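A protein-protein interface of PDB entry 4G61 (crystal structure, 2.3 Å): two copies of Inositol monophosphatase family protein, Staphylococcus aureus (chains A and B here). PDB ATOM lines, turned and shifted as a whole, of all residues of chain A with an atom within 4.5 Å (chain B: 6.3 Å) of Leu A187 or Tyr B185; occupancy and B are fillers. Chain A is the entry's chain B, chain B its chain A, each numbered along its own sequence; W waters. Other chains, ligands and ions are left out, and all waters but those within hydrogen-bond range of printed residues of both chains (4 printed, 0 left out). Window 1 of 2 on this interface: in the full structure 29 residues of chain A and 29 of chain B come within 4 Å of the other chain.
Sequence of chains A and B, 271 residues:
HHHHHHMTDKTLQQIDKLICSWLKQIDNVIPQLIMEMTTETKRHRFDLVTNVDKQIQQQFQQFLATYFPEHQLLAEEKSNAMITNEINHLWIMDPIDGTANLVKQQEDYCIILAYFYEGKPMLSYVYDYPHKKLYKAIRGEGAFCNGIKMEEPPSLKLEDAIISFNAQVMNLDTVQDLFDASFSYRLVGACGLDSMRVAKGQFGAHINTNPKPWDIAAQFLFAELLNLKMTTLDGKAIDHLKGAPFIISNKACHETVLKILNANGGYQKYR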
ATOM      1  N   SER A 164     -12.471  -9.637  11.620  1.00  0.00           N
ATOM      2  CA  SER A 164     -13.502  -9.960  10.626  1.00  0.00           C
ATOM      3  C   SER A 164     -13.472 -11.428  10.252  1.00  0.00           C
ATOM      4  O   SER A 164     -12.423 -12.002   9.991  1.00  0.00           O
ATOM      5  CB  SER A 164     -13.297  -9.068   9.382  1.00  0.00           C
ATOM      6  OG  SER A 164     -13.530  -9.720   8.149  1.00  0.00           O
ATOM      7  N   PHE A 165     -14.659 -12.003  10.162  1.00  0.00           N
ATOM      8  CA  PHE A 165     -14.852 -13.385   9.808  1.00  0.00           C
ATOM      9  C   PHE A 165     -16.335 -13.694   9.667  1.00  0.00           C
ATOM     10  O   PHE A 165     -17.180 -12.928  10.130  1.00  0.00           O
ATOM     11  CB  PHE A 165     -14.225 -14.277  10.866  1.00  0.00           C
ATOM     12  CG  PHE A 165     -14.830 -14.142  12.240  1.00  0.00           C
ATOM     13  CD1 PHE A 165     -15.884 -14.966  12.636  1.00  0.00           C
ATOM     14  CD2 PHE A 165     -14.285 -13.261  13.167  1.00  0.00           C
ATOM     15  CE1 PHE A 165     -16.400 -14.881  13.936  1.00  0.00           C
ATOM     16  CE2 PHE A 165     -14.795 -13.164  14.456  1.00  0.00           C
ATOM     17  CZ  PHE A 165     -15.846 -13.978  14.845  1.00  0.00           C
ATOM     18  N   GLN A 168     -21.252 -17.408  10.745  1.00  0.00           N
ATOM     19  CA  GLN A 168     -22.253 -18.471  10.517  1.00  0.00           C
ATOM     20  C   GLN A 168     -21.650 -19.893  10.283  1.00  0.00           C
ATOM     21  O   GLN A 168     -22.382 -20.901  10.297  1.00  0.00           O
ATOM     22  CB  GLN A 168     -23.175 -18.145   9.317  1.00  0.00           C
ATOM     23  CG  GLN A 168     -23.571 -16.664   9.170  1.00  0.00           C
ATOM     24  CD  GLN A 168     -24.457 -16.414   7.939  1.00  0.00           C
ATOM     25  OE1 GLN A 168     -24.659 -15.248   7.542  1.00  0.00           O
ATOM     26  NE2 GLN A 168     -24.960 -17.517   7.308  1.00  0.00           N
ATOM     27  N   TYR A 185     -15.912  -6.423  16.353  1.00  0.00           N
ATOM     28  CA  TYR A 185     -16.100  -7.272  15.182  1.00  0.00           C
ATOM     29  C   TYR A 185     -16.816  -6.479  14.086  1.00  0.00           C
ATOM     30  O   TYR A 185     -17.764  -5.751  14.370  1.00  0.00           O
ATOM     31  CB  TYR A 185     -16.829  -8.577  15.582  1.00  0.00           C
ATOM     32  CG  TYR A 185     -17.410  -9.394  14.454  1.00  0.00           C
ATOM     33  CD1 TYR A 185     -16.637 -10.281  13.741  1.00  0.00           C
ATOM     34  CD2 TYR A 185     -18.777  -9.345  14.150  1.00  0.00           C
ATOM     35  CE1 TYR A 185     -17.167 -11.033  12.685  1.00  0.00           C
ATOM     36  CE2 TYR A 185     -19.333 -10.170  13.106  1.00  0.00           C
ATOM     37  CZ  TYR A 185     -18.504 -11.004  12.388  1.00  0.00           C
ATOM     38  OH  TYR A 185     -19.002 -11.790  11.350  1.00  0.00           O
ATOM     39  N   ARG A 186     -16.305  -6.555  12.862  1.00  0.00           N
ATOM     40  CA  ARG A 186     -16.983  -5.987  11.691  1.00  0.00           C
ATOM     41  C   ARG A 186     -16.933  -7.060  10.581  1.00  0.00           C
ATOM     42  O   ARG A 186     -16.149  -8.003  10.653  1.00  0.00           O
ATOM     43  CB  ARG A 186     -16.278  -4.727  11.144  1.00  0.00           C
ATOM     44  CG  ARG A 186     -15.938  -3.524  12.076  1.00  0.00           C
ATOM     45  CD  ARG A 186     -17.090  -2.504  12.305  1.00  0.00           C
ATOM     46  NE  ARG A 186     -17.560  -2.941  13.546  1.00  0.00           N
ATOM     47  CZ  ARG A 186     -17.439  -2.356  14.715  1.00  0.00           C
ATOM     48  NH1 ARG A 186     -16.966  -1.136  14.896  1.00  0.00           N
ATOM     49  NH2 ARG A 186     -17.850  -3.075  15.714  1.00  0.00           N
ATOM     50  N   LEU A 187     -17.702  -6.880   9.525  1.00  0.00           N
ATOM     51  CA  LEU A 187     -17.548  -7.692   8.332  1.00  0.00           C
ATOM     52  C   LEU A 187     -17.915  -6.931   7.052  1.00  0.00           C
ATOM     53  O   LEU A 187     -19.014  -6.345   6.973  1.00  0.00           O
ATOM     54  CB  LEU A 187     -18.425  -8.915   8.422  1.00  0.00           C
ATOM     55  CG  LEU A 187     -18.370  -9.849   7.221  1.00  0.00           C
ATOM     56  CD1 LEU A 187     -16.939 -10.454   7.009  1.00  0.00           C
ATOM     57  CD2 LEU A 187     -19.385 -10.933   7.472  1.00  0.00           C
ATOM     58  N   VAL A 188     -16.994  -6.924   6.075  1.00  0.00           N
ATOM     59  CA  VAL A 188     -17.287  -6.335   4.757  1.00  0.00           C
ATOM     60  C   VAL A 188     -18.045  -7.311   3.826  1.00  0.00           C
ATOM     61  O   VAL A 188     -19.020  -6.950   3.119  1.00  0.00           O
ATOM     62  CB  VAL A 188     -16.021  -5.717   4.088  1.00  0.00           C
ATOM     63  CG1 VAL A 188     -16.344  -5.130   2.742  1.00  0.00           C
ATOM     64  CG2 VAL A 188     -15.422  -4.636   4.958  1.00  0.00           C
ATOM     65  N   GLY A 189     -17.647  -8.570   3.853  1.00  0.00           N
ATOM     66  CA  GLY A 189     -18.374  -9.553   3.087  1.00  0.00           C
ATOM     67  C   GLY A 189     -17.694  -9.894   1.764  1.00  0.00           C
ATOM     68  O   GLY A 189     -18.300 -10.596   0.936  1.00  0.00           O
ATOM     69  N   ASP A 194     -12.045  -7.451   2.954  1.00  0.00           N
ATOM     70  CA  ASP A 194     -11.725  -7.699   4.366  1.00  0.00           C
ATOM     71  C   ASP A 194     -10.214  -7.898   4.556  1.00  0.00           C
ATOM     72  O   ASP A 194      -9.654  -7.420   5.544  1.00  0.00           O
ATOM     73  CB  ASP A 194     -12.465  -8.930   4.917  1.00  0.00           C
ATOM     74  CG  ASP A 194     -13.964  -8.678   5.142  1.00  0.00           C
ATOM     75  OD1 ASP A 194     -14.300  -7.991   6.131  1.00  0.00           O
ATOM     76  OD2 ASP A 194     -14.803  -9.202   4.359  1.00  0.00           O
ATOM     77  N   ALA B 161     -32.608 -11.175   2.151  1.00  0.00           N
ATOM     78  CA  ALA B 161     -32.001  -9.925   2.623  1.00  0.00           C
ATOM     79  C   ALA B 161     -30.783 -10.088   3.577  1.00  0.00           C
ATOM     80  O   ALA B 161     -30.708 -11.011   4.424  1.00  0.00           O
ATOM     81  CB  ALA B 161     -33.064  -9.072   3.291  1.00  0.00           C
ATOM     82  N   ILE B 162     -29.841  -9.165   3.438  1.00  0.00           N
ATOM     83  CA  ILE B 162     -28.719  -9.127   4.329  1.00  0.00           C
ATOM     84  C   ILE B 162     -29.163  -8.324   5.515  1.00  0.00           C
ATOM     85  O   ILE B 162     -29.887  -7.346   5.335  1.00  0.00           O
ATOM     86  CB  ILE B 162     -27.586  -8.397   3.653  1.00  0.00           C
ATOM     87  CG1 ILE B 162     -26.973  -9.278   2.539  1.00  0.00           C
ATOM     88  CG2 ILE B 162     -26.608  -7.887   4.681  1.00  0.00           C
ATOM     89  CD1 ILE B 162     -25.904  -8.507   1.688  1.00  0.00           C
ATOM     90  N   ILE B 163     -28.759  -8.733   6.724  1.00  0.00           N
ATOM     91  CA  ILE B 163     -29.022  -7.921   7.909  1.00  0.00           C
ATOM     92  C   ILE B 163     -27.817  -7.595   8.752  1.00  0.00           C
ATOM     93  O   ILE B 163     -26.773  -8.234   8.683  1.00  0.00           O
ATOM     94  CB  ILE B 163     -30.072  -8.516   8.824  1.00  0.00           C
ATOM     95  CG1 ILE B 163     -29.719  -9.947   9.216  1.00  0.00           C
ATOM     96  CG2 ILE B 163     -31.445  -8.447   8.126  1.00  0.00           C
ATOM     97  CD1 ILE B 163     -30.554 -10.392  10.375  1.00  0.00           C
ATOM     98  N   SER B 164     -27.978  -6.543   9.523  1.00  0.00           N
ATOM     99  CA  SER B 164     -26.920  -6.019  10.316  1.00  0.00           C
ATOM    100  C   SER B 164     -27.401  -5.813  11.770  1.00  0.00           C
ATOM    101  O   SER B 164     -28.519  -5.349  12.013  1.00  0.00           O
ATOM    102  CB  SER B 164     -26.463  -4.748   9.635  1.00  0.00           C
ATOM    103  OG  SER B 164     -26.304  -3.693  10.511  1.00  0.00           O
ATOM    104  N   PHE B 165     -26.574  -6.205  12.735  1.00  0.00           N
ATOM    105  CA  PHE B 165     -26.853  -5.920  14.156  1.00  0.00           C
ATOM    106  C   PHE B 165     -25.568  -6.211  14.866  1.00  0.00           C
ATOM    107  O   PHE B 165     -24.654  -6.802  14.258  1.00  0.00           O
ATOM    108  CB  PHE B 165     -27.953  -6.834  14.738  1.00  0.00           C
ATOM    109  CG  PHE B 165     -27.742  -8.326  14.464  1.00  0.00           C
ATOM    110  CD1 PHE B 165     -27.120  -9.155  15.411  1.00  0.00           C
ATOM    111  CD2 PHE B 165     -28.206  -8.901  13.276  1.00  0.00           C
ATOM    112  CE1 PHE B 165     -26.950 -10.557  15.153  1.00  0.00           C
ATOM    113  CE2 PHE B 165     -28.037 -10.273  13.001  1.00  0.00           C
ATOM    114  CZ  PHE B 165     -27.387 -11.085  13.935  1.00  0.00           C
ATOM    115  N   ASN B 166     -25.495  -5.811  16.144  1.00  0.00           N
ATOM    116  CA  ASN B 166     -24.348  -6.104  16.982  1.00  0.00           C
ATOM    117  C   ASN B 166     -24.518  -7.501  17.567  1.00  0.00           C
ATOM    118  O   ASN B 166     -25.364  -7.715  18.412  1.00  0.00           O
ATOM    119  CB  ASN B 166     -24.218  -5.044  18.087  1.00  0.00           C
ATOM    120  CG  ASN B 166     -22.958  -5.244  18.953  1.00  0.00           C
ATOM    121  OD1 ASN B 166     -22.318  -6.282  18.884  1.00  0.00           O
ATOM    122  ND2 ASN B 166     -22.634  -4.260  19.795  1.00  0.00           N
ATOM    123  N   ALA B 167     -23.731  -8.466  17.110  1.00  0.00           N
ATOM    124  CA  ALA B 167     -23.949  -9.838  17.519  1.00  0.00           C
ATOM    125  C   ALA B 167     -23.286 -10.102  18.862  1.00  0.00           C
ATOM    126  O   ALA B 167     -23.365 -11.202  19.373  1.00  0.00           O
ATOM    127  CB  ALA B 167     -23.458 -10.817  16.455  1.00  0.00           C
ATOM    128  N   GLN B 168     -22.625  -9.093  19.446  1.00  0.00           N
ATOM    129  CA  GLN B 168     -21.868  -9.298  20.701  1.00  0.00           C
ATOM    130  C   GLN B 168     -22.716  -9.066  21.939  1.00  0.00           C
ATOM    131  O   GLN B 168     -22.290  -9.396  23.058  1.00  0.00           O
ATOM    132  CB  GLN B 168     -20.663  -8.369  20.751  1.00  0.00           C
ATOM    133  CG  GLN B 168     -19.734  -8.575  19.547  1.00  0.00           C
ATOM    134  CD  GLN B 168     -18.410  -7.871  19.711  1.00  0.00           C
ATOM    135  OE1 GLN B 168     -18.001  -7.111  18.865  1.00  0.00           O
ATOM    136  NE2 GLN B 168     -17.759  -8.120  20.801  1.00  0.00           N
ATOM    137  N   PHE B 179     -29.244 -15.378  11.840  1.00  0.00           N
ATOM    138  CA  PHE B 179     -28.398 -15.920  10.754  1.00  0.00           C
ATOM    139  C   PHE B 179     -29.149 -16.876   9.862  1.00  0.00           C
ATOM    140  O   PHE B 179     -29.036 -16.791   8.633  1.00  0.00           O
ATOM    141  CB  PHE B 179     -27.199 -16.703  11.305  1.00  0.00           C
ATOM    142  CG  PHE B 179     -26.114 -15.846  11.958  1.00  0.00           C
ATOM    143  CD1 PHE B 179     -26.043 -14.452  11.747  1.00  0.00           C
ATOM    144  CD2 PHE B 179     -25.093 -16.471  12.724  1.00  0.00           C
ATOM    145  CE1 PHE B 179     -25.028 -13.691  12.310  1.00  0.00           C
ATOM    146  CE2 PHE B 179     -24.046 -15.717  13.282  1.00  0.00           C
ATOM    147  CZ  PHE B 179     -24.022 -14.300  13.072  1.00  0.00           C
ATOM    148  N   SER B 182     -32.005 -15.187   7.504  1.00  0.00           N
ATOM    149  CA  SER B 182     -31.716 -14.147   6.539  1.00  0.00           C
ATOM    150  C   SER B 182     -30.796 -14.641   5.428  1.00  0.00           C
ATOM    151  O   SER B 182     -30.277 -15.764   5.502  1.00  0.00           O
ATOM    152  CB  SER B 182     -31.130 -12.943   7.251  1.00  0.00           C
ATOM    153  OG  SER B 182     -30.001 -13.369   7.938  1.00  0.00           O
ATOM    154  N   PHE B 183     -30.582 -13.818   4.403  1.00  0.00           N
ATOM    155  CA  PHE B 183     -29.754 -14.242   3.301  1.00  0.00           C
ATOM    156  C   PHE B 183     -28.301 -14.310   3.752  1.00  0.00           C
ATOM    157  O   PHE B 183     -27.595 -15.249   3.451  1.00  0.00           O
ATOM    158  CB  PHE B 183     -29.901 -13.326   2.093  1.00  0.00           C
ATOM    159  CG  PHE B 183     -29.217 -13.860   0.864  1.00  0.00           C
ATOM    160  CD1 PHE B 183     -29.904 -14.713  -0.014  1.00  0.00           C
ATOM    161  CD2 PHE B 183     -27.871 -13.547   0.606  1.00  0.00           C
ATOM    162  CE1 PHE B 183     -29.276 -15.241  -1.140  1.00  0.00           C
ATOM    163  CE2 PHE B 183     -27.230 -14.067  -0.514  1.00  0.00           C
ATOM    164  CZ  PHE B 183     -27.941 -14.926  -1.392  1.00  0.00           C
ATOM    165  N   SER B 184     -27.881 -13.293   4.488  1.00  0.00           N
ATOM    166  CA  SER B 184     -26.546 -13.249   5.078  1.00  0.00           C
ATOM    167  C   SER B 184     -26.452 -12.093   6.086  1.00  0.00           C
ATOM    168  O   SER B 184     -27.423 -11.342   6.289  1.00  0.00           O
ATOM    169  CB  SER B 184     -25.495 -13.050   4.004  1.00  0.00           C
ATOM    170  OG  SER B 184     -24.273 -13.409   4.553  1.00  0.00           O
ATOM    171  N   TYR B 185     -25.278 -11.953   6.681  1.00  0.00           N
ATOM    172  CA  TYR B 185     -25.018 -10.944   7.664  1.00  0.00           C
ATOM    173  C   TYR B 185     -23.800 -10.058   7.320  1.00  0.00           C
ATOM    174  O   TYR B 185     -22.791 -10.535   6.789  1.00  0.00           O
ATOM    175  CB  TYR B 185     -24.783 -11.656   8.977  1.00  0.00           C
ATOM    176  CG  TYR B 185     -24.271 -10.794  10.107  1.00  0.00           C
ATOM    177  CD1 TYR B 185     -25.143 -10.151  10.979  1.00  0.00           C
ATOM    178  CD2 TYR B 185     -22.886 -10.654  10.314  1.00  0.00           C
ATOM    179  CE1 TYR B 185     -24.625  -9.361  12.047  1.00  0.00           C
ATOM    180  CE2 TYR B 185     -22.364  -9.881  11.355  1.00  0.00           C
ATOM    181  CZ  TYR B 185     -23.232  -9.236  12.231  1.00  0.00           C
ATOM    182  OH  TYR B 185     -22.671  -8.497  13.272  1.00  0.00           O
ATOM    183  N   ARG B 186     -23.902  -8.769   7.650  1.00  0.00           N
ATOM    184  CA  ARG B 186     -22.815  -7.820   7.445  1.00  0.00           C
ATOM    185  C   ARG B 186     -22.900  -6.772   8.571  1.00  0.00           C
ATOM    186  O   ARG B 186     -23.928  -6.652   9.223  1.00  0.00           O
ATOM    187  CB  ARG B 186     -22.949  -7.074   6.107  1.00  0.00           C
ATOM    188  CG  ARG B 186     -23.310  -7.826   4.831  1.00  0.00           C
ATOM    189  CD  ARG B 186     -22.059  -8.300   4.038  1.00  0.00           C
ATOM    190  NE  ARG B 186     -22.053  -9.702   4.315  1.00  0.00           N
ATOM    191  CZ  ARG B 186     -22.108 -10.742   3.504  1.00  0.00           C
ATOM    192  NH1 ARG B 186     -22.039 -10.694   2.180  1.00  0.00           N
ATOM    193  NH2 ARG B 186     -22.192 -11.888   4.132  1.00  0.00           N
ATOM    194  N   LEU B 187     -21.821  -6.036   8.801  1.00  0.00           N
ATOM    195  CA  LEU B 187     -21.815  -4.984   9.828  1.00  0.00           C
ATOM    196  C   LEU B 187     -20.866  -3.855   9.468  1.00  0.00           C
ATOM    197  O   LEU B 187     -19.640  -4.085   9.350  1.00  0.00           O
ATOM    198  CB  LEU B 187     -21.434  -5.539  11.202  1.00  0.00           C
ATOM    199  CG  LEU B 187     -21.565  -4.456  12.297  1.00  0.00           C
ATOM    200  CD1 LEU B 187     -23.037  -3.853  12.376  1.00  0.00           C
ATOM    201  CD2 LEU B 187     -21.079  -4.966  13.682  1.00  0.00           C
ATOM    202  N   VAL B 188     -21.412  -2.653   9.273  1.00  0.00           N
ATOM    203  CA  VAL B 188     -20.549  -1.470   9.037  1.00  0.00           C
ATOM    204  C   VAL B 188     -19.977  -0.966  10.411  1.00  0.00           C
ATOM    205  O   VAL B 188     -18.800  -0.632  10.496  1.00  0.00           O
ATOM    206  CB  VAL B 188     -21.287  -0.316   8.322  1.00  0.00           C
ATOM    207  CG1 VAL B 188     -20.323   0.828   7.996  1.00  0.00           C
ATOM    208  CG2 VAL B 188     -21.961  -0.767   7.017  1.00  0.00           C
HETATM  209  O   HOH W   1     -19.571  -6.003  16.559  1.00  0.00           O
HETATM  210  O   HOH W   2     -27.620 -14.805   7.455  1.00  0.00           O
HETATM  211  O   HOH W   3     -20.411 -10.995  -0.637  1.00  0.00           O
HETATM  212  O   HOH W   4     -22.025 -13.113   7.370  1.00  0.00           O
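N of Leu B187 is in hydrogen-bond range of O of Leu A187 (3.4 Å).
The backbone NH (N) of Tyr B185 is in hydrogen-bond range of the side-chain amide oxygen (OE1) of Gln A168 (3.5 Å).
OE1 of Gln B168 lies within hydrogen-bond range of N of Tyr A185 (3.3 Å).
The backbone carbonyl oxygen (O) of Ser B184 is in hydrogen-bond range of the backbone NH (N) of Ile B163.
The backbone carbonyl oxygen (O) of Phe B165 sits at hydrogen-bond distance from the side-chain hydroxyl (OH) of Tyr B185 (2.8 Å).
The side-chain carboxylate of Asp A194 is in hydrogen-bond range of the backbone NH of Val A188, 2.9 Å away.
The backbone NH (N) of Gln B168 lies within hydrogen-bond range of the side-chain amide oxygen (OD1) of Asn B166 (2.9 Å).
The side-chain carboxylate (OD2) of Asp A194 sits at hydrogen-bond distance from the backbone NH (N) of Gly A189 (3.0 Å).
The side-chain hydroxyl (OG) of Ser B184 is in hydrogen-bond range of the guanidinium group (NH2) of Arg B186 (2.6 Å).
Among the printed residues, merely in contact across the chains: Gln A168 with Phe B179 (3.9 Å), Gln A168 with Ser B184 (3.5 Å), Tyr A185 with Tyr B185 (3.5 Å), Tyr A185 with Leu B187 (3.5 Å), Arg A186 with Leu B187 (3.9 Å), Arg A186 with Val B188 (3.1 Å), Leu A187 with Tyr B185 (3.5 Å), Val A188 with Arg B186 (3.5 Å) and Gly A189 with Arg B186 (3.9 Å).
Of the printed residues of chain B, Gln A168 touches Phe B179, Ser B184 and Tyr B185.
Of chain B, only Tyr B185 and Leu B187 come within 4 Å of Leu A187.
Asp A194 touches none of the printed residues of chain B.
Ile B163 touches none of the printed residues of chain A.
Of chain A, only Gln A168, Tyr A185 and Leu A187 come within 4 Å of Tyr B185.
Printed residues of chain A within 4 Å of Leu B187: Tyr A185, Arg A186 and Leu A187.
The nearest residue of chain B that does not touch Leu A187 is Arg B186 (4.1 Å).
Of the 9 printed residues of chain A, 6 touch a printed residue of chain B.
Of the 16 printed residues of chain B, 7 touch a printed residue of chain A.
Hydrophobic or aromatic side chains of chain B that line the printed part of chain A: Phe B179, Tyr B185 and Leu B187.
Among the printed residues, 12 pairs touch across the chains.
Among the printed residues, no Asp or Glu carboxylate lies within 4 Å of a Lys or Arg side-chain nitrogen of the other chain.
Gln A168 touches Tyr B185, and with the chains exchanged Tyr A185 touches Gln B168.
Tyr A185 touches its own counterpart, Tyr B185.
Arg A186 touches Leu B187, but with the chains exchanged Leu A187 does not touch Arg B186 (4.1 Å).
Arg A186 touches Val B188, and with the chains exchanged Val A188 touches Arg B186.
Of the 12 pairs that touch across the chains among the printed residues, 8 have their exchanged pair printed and touching as well.
Water W3 bridges the backbone carbonyl oxygen of Gly A189 (2.7 Å) and the guanidinium group of Arg B186 (3.3 Å).
Water W2 lies within hydrogen-bond range of the backbone carbonyl oxygen of Phe B179 (2.7 Å), the side-chain hydroxyl of Ser B182 (2.8 Å), the side-chain amide oxygen of Gln A168 (3.0 Å) and the backbone NH of Ser B184 (3.3 Å).
Water W4 lies within hydrogen-bond range of the backbone carbonyl oxygen (O) of Tyr B185 (2.8 Å), the side-chain amide oxygen (OE1) of Gln A168 (3.4 Å) and the guanidinium group (NH2) of Arg B186 (3.5 Å).
Water W1 bridges O of Tyr A185 (2.8 Å) and OE1 of Gln B168 (3.0 Å).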
